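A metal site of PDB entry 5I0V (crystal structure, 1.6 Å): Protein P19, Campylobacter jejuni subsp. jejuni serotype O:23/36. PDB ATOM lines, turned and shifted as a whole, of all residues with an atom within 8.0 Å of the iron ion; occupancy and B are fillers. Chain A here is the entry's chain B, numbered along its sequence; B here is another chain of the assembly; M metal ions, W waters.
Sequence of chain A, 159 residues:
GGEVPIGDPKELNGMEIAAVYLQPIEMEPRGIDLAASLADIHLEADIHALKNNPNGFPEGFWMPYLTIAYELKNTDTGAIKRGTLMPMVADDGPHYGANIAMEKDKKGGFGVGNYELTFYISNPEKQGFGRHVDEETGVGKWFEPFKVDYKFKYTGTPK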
ATOM      1  N   GLU A   3      13.661  20.345   7.609  1.00  0.00           N
ATOM      2  CA  GLU A   3      12.364  20.146   6.960  1.00  0.00           C
ATOM      3  C   GLU A   3      12.030  18.692   6.737  1.00  0.00           C
ATOM      4  O   GLU A   3      12.857  17.904   6.272  1.00  0.00           O
ATOM      5  CB  GLU A   3      12.299  20.920   5.651  1.00  0.00           C
ATOM      6  CG  GLU A   3      12.451  22.419   5.843  1.00  0.00           C
ATOM      7  CD  GLU A   3      12.195  23.183   4.564  1.00  0.00           C
ATOM      8  OE1 GLU A   3      12.224  22.555   3.491  1.00  0.00           O
ATOM      9  OE2 GLU A   3      11.950  24.415   4.624  1.00  0.00           O
ATOM     10  N   VAL A  20       6.101  20.591   3.087  1.00  0.00           N
ATOM     11  CA  VAL A  20       7.020  20.203   4.126  1.00  0.00           C
ATOM     12  C   VAL A  20       6.526  20.769   5.442  1.00  0.00           C
ATOM     13  O   VAL A  20       5.672  21.672   5.460  1.00  0.00           O
ATOM     14  CB  VAL A  20       8.474  20.713   3.899  1.00  0.00           C
ATOM     15  CG1 VAL A  20       9.061  20.196   2.579  1.00  0.00           C
ATOM     16  CG2 VAL A  20       8.575  22.257   3.963  1.00  0.00           C
ATOM     17  N   TYR A  21       7.036  20.222   6.550  1.00  0.00           N
ATOM     18  CA  TYR A  21       6.907  20.889   7.836  1.00  0.00           C
ATOM     19  C   TYR A  21       8.248  20.952   8.561  1.00  0.00           C
ATOM     20  O   TYR A  21       9.157  20.132   8.326  1.00  0.00           O
ATOM     21  CB  TYR A  21       5.802  20.290   8.691  1.00  0.00           C
ATOM     22  CG  TYR A  21       6.069  18.930   9.296  1.00  0.00           C
ATOM     23  CD1 TYR A  21       6.615  18.818  10.574  1.00  0.00           C
ATOM     24  CD2 TYR A  21       5.730  17.779   8.622  1.00  0.00           C
ATOM     25  CE1 TYR A  21       6.879  17.580  11.133  1.00  0.00           C
ATOM     26  CE2 TYR A  21       5.965  16.531   9.171  1.00  0.00           C
ATOM     27  CZ  TYR A  21       6.533  16.438  10.441  1.00  0.00           C
ATOM     28  OH  TYR A  21       6.777  15.207  11.022  1.00  0.00           O
ATOM     29  N   LEU A  22       8.372  21.955   9.407  1.00  0.00           N
ATOM     30  CA  LEU A  22       9.535  22.106  10.235  1.00  0.00           C
ATOM     31  C   LEU A  22       9.074  22.585  11.621  1.00  0.00           C
ATOM     32  O   LEU A  22       7.877  22.583  11.910  1.00  0.00           O
ATOM     33  CB  LEU A  22      10.546  23.070   9.605  1.00  0.00           C
ATOM     34  CG  LEU A  22      10.061  24.491   9.248  1.00  0.00           C
ATOM     35  CD1 LEU A  22      11.214  25.491   9.257  1.00  0.00           C
ATOM     36  CD2 LEU A  22       9.354  24.524   7.898  1.00  0.00           C
ATOM     37  N   HIS A  42       5.722  24.363  11.588  1.00  0.00           N
ATOM     38  CA  HIS A  42       5.494  25.349  10.544  1.00  0.00           C
ATOM     39  C   HIS A  42       5.250  24.524   9.314  1.00  0.00           C
ATOM     40  O   HIS A  42       6.101  23.735   8.936  1.00  0.00           O
ATOM     41  CB  HIS A  42       6.698  26.282  10.380  1.00  0.00           C
ATOM     42  CG  HIS A  42       6.393  27.517   9.525  1.00  0.00           C
ATOM     43  ND1 HIS A  42       5.417  28.394   9.848  1.00  0.00           N
ATOM     44  CD2 HIS A  42       6.968  27.987   8.347  1.00  0.00           C
ATOM     45  CE1 HIS A  42       5.376  29.385   8.944  1.00  0.00           C
ATOM     46  NE2 HIS A  42       6.324  29.143   8.026  1.00  0.00           N
ATOM     47  N   LEU A  43       4.068  24.679   8.694  1.00  0.00           N
ATOM     48  CA  LEU A  43       3.717  23.992   7.477  1.00  0.00           C
ATOM     49  C   LEU A  43       4.001  24.928   6.304  1.00  0.00           C
ATOM     50  O   LEU A  43       3.611  26.080   6.350  1.00  0.00           O
ATOM     51  CB  LEU A  43       2.230  23.639   7.490  1.00  0.00           C
ATOM     52  CG  LEU A  43       1.621  23.108   6.170  1.00  0.00           C
ATOM     53  CD1 LEU A  43       2.244  21.758   5.878  1.00  0.00           C
ATOM     54  CD2 LEU A  43       0.110  22.953   6.320  1.00  0.00           C
ATOM     55  N   GLU A  44       4.658  24.406   5.287  1.00  0.00           N
ATOM     56  CA  GLU A  44       4.985  25.195   4.105  1.00  0.00           C
ATOM     57  C   GLU A  44       4.506  24.527   2.818  1.00  0.00           C
ATOM     58  O   GLU A  44       4.585  23.286   2.671  1.00  0.00           O
ATOM     59  CB  GLU A  44       6.500  25.406   4.000  1.00  0.00           C
ATOM     60  CG  GLU A  44       7.068  26.223   5.141  1.00  0.00           C
ATOM     61  CD  GLU A  44       8.541  26.466   5.026  1.00  0.00           C
ATOM     62  OE1 GLU A  44       9.246  25.773   4.236  1.00  0.00           O
ATOM     63  OE2 GLU A  44       9.032  27.352   5.757  1.00  0.00           O
ATOM     64  N   ALA A  45       3.963  25.350   1.929  1.00  0.00           N
ATOM     65  CA  ALA A  45       3.689  24.911   0.569  1.00  0.00           C
ATOM     66  C   ALA A  45       4.795  25.529  -0.265  1.00  0.00           C
ATOM     67  O   ALA A  45       4.996  26.751  -0.233  1.00  0.00           O
ATOM     68  CB  ALA A  45       2.318  25.371   0.092  1.00  0.00           C
ATOM     69  N   ASP A  46       5.530  24.663  -0.961  1.00  0.00           N
ATOM     70  CA  ASP A  46       6.619  25.080  -1.849  1.00  0.00           C
ATOM     71  C   ASP A  46       6.179  24.929  -3.286  1.00  0.00           C
ATOM     72  O   ASP A  46       5.959  23.809  -3.763  1.00  0.00           O
ATOM     73  CB  ASP A  46       7.869  24.219  -1.609  1.00  0.00           C
ATOM     74  CG  ASP A  46       8.605  24.594  -0.334  1.00  0.00           C
ATOM     75  OD1 ASP A  46       8.628  25.798   0.037  1.00  0.00           O
ATOM     76  OD2 ASP A  46       9.139  23.679   0.312  1.00  0.00           O
ATOM     77  N   ALA A  90      11.825  33.156   4.074  1.00  0.00           N
ATOM     78  CA  ALA A  90      12.728  32.587   5.081  1.00  0.00           C
ATOM     79  C   ALA A  90      14.085  32.508   4.431  1.00  0.00           C
ATOM     80  O   ALA A  90      14.272  32.980   3.304  1.00  0.00           O
ATOM     81  CB  ALA A  90      12.240  31.205   5.499  1.00  0.00           C
ATOM     82  N   ASP A  91      15.051  31.902   5.139  1.00  0.00           N
ATOM     83  CA  ASP A  91      16.408  31.777   4.630  1.00  0.00           C
ATOM     84  C   ASP A  91      16.462  31.018   3.318  1.00  0.00           C
ATOM     85  O   ASP A  91      17.341  31.274   2.489  1.00  0.00           O
ATOM     86  CB  ASP A  91      17.316  31.128   5.683  1.00  0.00           C
ATOM     87  CG  ASP A  91      16.896  29.711   6.052  1.00  0.00           C
ATOM     88  OD1 ASP A  91      15.748  29.293   5.786  1.00  0.00           O
ATOM     89  OD2 ASP A  91      17.722  29.009   6.654  1.00  0.00           O
ATOM     90  N   ASP A  92      15.507  30.107   3.117  1.00  0.00           N
ATOM     91  CA  ASP A  92      15.419  29.301   1.897  1.00  0.00           C
ATOM     92  C   ASP A  92      14.460  29.916   0.851  1.00  0.00           C
ATOM     93  O   ASP A  92      14.009  29.235  -0.085  1.00  0.00           O
ATOM     94  CB  ASP A  92      15.053  27.829   2.238  1.00  0.00           C
ATOM     95  CG  ASP A  92      13.634  27.658   2.767  1.00  0.00           C
ATOM     96  OD1 ASP A  92      13.026  28.643   3.227  1.00  0.00           O
ATOM     97  OD2 ASP A  92      13.090  26.525   2.720  1.00  0.00           O
ATOM     98  N   GLY A  93      14.171  31.210   1.019  1.00  0.00           N
ATOM     99  CA  GLY A  93      13.398  31.982   0.056  1.00  0.00           C
ATOM    100  C   GLY A  93      11.905  32.045   0.321  1.00  0.00           C
ATOM    101  O   GLY A  93      11.441  31.585   1.366  1.00  0.00           O
ATOM    102  N   PRO A  94      11.153  32.622  -0.616  1.00  0.00           N
ATOM    103  CA  PRO A  94       9.721  32.835  -0.438  1.00  0.00           C
ATOM    104  C   PRO A  94       8.936  31.521  -0.465  1.00  0.00           C
ATOM    105  O   PRO A  94       9.334  30.549  -1.149  1.00  0.00           O
ATOM    106  CB  PRO A  94       9.345  33.733  -1.623  1.00  0.00           C
ATOM    107  CG  PRO A  94      10.357  33.411  -2.683  1.00  0.00           C
ATOM    108  CD  PRO A  94      11.635  33.129  -1.931  1.00  0.00           C
ATOM    109  N   HIS A  95       7.860  31.467   0.312  1.00  0.00           N
ATOM    110  CA  HIS A  95       6.955  30.318   0.312  1.00  0.00           C
ATOM    111  C   HIS A  95       5.632  30.734   0.867  1.00  0.00           C
ATOM    112  O   HIS A  95       5.398  31.914   1.178  1.00  0.00           O
ATOM    113  CB  HIS A  95       7.534  29.188   1.168  1.00  0.00           C
ATOM    114  CG  HIS A  95       7.780  29.613   2.601  1.00  0.00           C
ATOM    115  ND1 HIS A  95       8.932  30.208   2.981  1.00  0.00           N
ATOM    116  CD2 HIS A  95       6.972  29.529   3.731  1.00  0.00           C
ATOM    117  CE1 HIS A  95       8.865  30.487   4.309  1.00  0.00           C
ATOM    118  NE2 HIS A  95       7.661  30.081   4.754  1.00  0.00           N
ATOM    119  N   TYR A  96       4.738  29.771   1.021  1.00  0.00           N
ATOM    120  CA  TYR A  96       3.489  30.004   1.733  1.00  0.00           C
ATOM    121  C   TYR A  96       3.507  29.140   2.975  1.00  0.00           C
ATOM    122  O   TYR A  96       3.781  27.954   2.890  1.00  0.00           O
ATOM    123  CB  TYR A  96       2.281  29.656   0.870  1.00  0.00           C
ATOM    124  CG  TYR A  96       2.195  30.445  -0.424  1.00  0.00           C
ATOM    125  CD1 TYR A  96       1.480  31.635  -0.491  1.00  0.00           C
ATOM    126  CD2 TYR A  96       2.817  29.973  -1.593  1.00  0.00           C
ATOM    127  CE1 TYR A  96       1.372  32.355  -1.669  1.00  0.00           C
ATOM    128  CE2 TYR A  96       2.702  30.703  -2.789  1.00  0.00           C
ATOM    129  CZ  TYR A  96       1.986  31.874  -2.819  1.00  0.00           C
ATOM    130  OH  TYR A  96       1.906  32.583  -4.008  1.00  0.00           O
ATOM    131  N   HIS B 132      10.518  35.361   8.242  1.00  0.00           N
ATOM    132  CA  HIS B 132      10.979  34.634   9.405  1.00  0.00           C
ATOM    133  C   HIS B 132      12.047  35.461  10.059  1.00  0.00           C
ATOM    134  O   HIS B 132      12.893  36.041   9.383  1.00  0.00           O
ATOM    135  CB  HIS B 132      11.573  33.288   9.014  1.00  0.00           C
ATOM    136  CG  HIS B 132      10.571  32.283   8.465  1.00  0.00           C
ATOM    137  ND1 HIS B 132      10.799  30.955   8.536  1.00  0.00           N
ATOM    138  CD2 HIS B 132       9.346  32.429   7.819  1.00  0.00           C
ATOM    139  CE1 HIS B 132       9.789  30.288   7.952  1.00  0.00           C
ATOM    140  NE2 HIS B 132       8.877  31.186   7.540  1.00  0.00           N
ATOM    141  N   THR B 137      15.971  30.053  10.893  1.00  0.00           N
ATOM    142  CA  THR B 137      15.468  30.223   9.518  1.00  0.00           C
ATOM    143  C   THR B 137      15.259  31.671   9.109  1.00  0.00           C
ATOM    144  O   THR B 137      14.793  31.933   7.976  1.00  0.00           O
ATOM    145  CB  THR B 137      14.136  29.471   9.287  1.00  0.00           C
ATOM    146  OG1 THR B 137      13.074  30.133   9.991  1.00  0.00           O
ATOM    147  CG2 THR B 137      14.219  28.016   9.729  1.00  0.00           C
HETATM  148 FE    FE M   1      11.107  25.830   3.437  1.00  0.00          FE
HETATM  149 CU    CU M   2       7.067  30.489   6.701  1.00  0.00          CU
HETATM  150  O   HOH W   1      10.159  27.058   1.976  1.00  0.00           O
HETATM  151  O   HOH W   2      11.533  27.440   5.006  1.00  0.00           O
HETATM  152  O   HOH W   3      10.972  24.342   1.989  1.00  0.00           O
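Of the 18 residues printed, 3 come within 4 Å of the iron ion.
The iron ion is bound by OE1 of Glu 44 (2.0 Å). OE2 of Glu 3 binds the iron ion (2.0 Å). Water W3 binds the iron ion, 2.1 Å away. Water W1 binds the iron ion (2.1 Å). OD2 of Asp 92 binds the iron ion (2.2 Å). Water W2 binds the iron ion (2.3 Å).
The backbone NH (N) of Glu 44 is in hydrogen-bond range of the backbone carbonyl oxygen (O) of Val 20 (2.9 Å). The side-chain carboxylate (OE2) of Glu 44 lies close to a ring nitrogen (NE2) of His 95 (3.2 Å).
Water W2 lies within hydrogen-bond range of the side-chain carboxylate (OE2) of Glu 44 (2.6 Å) and the side-chain carboxylate (OD1) of Asp 92 (2.6 Å). Water W3 bridges OD2 of Asp 46 (2.6 Å) and OE1 of Glu 3 (2.6 Å).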
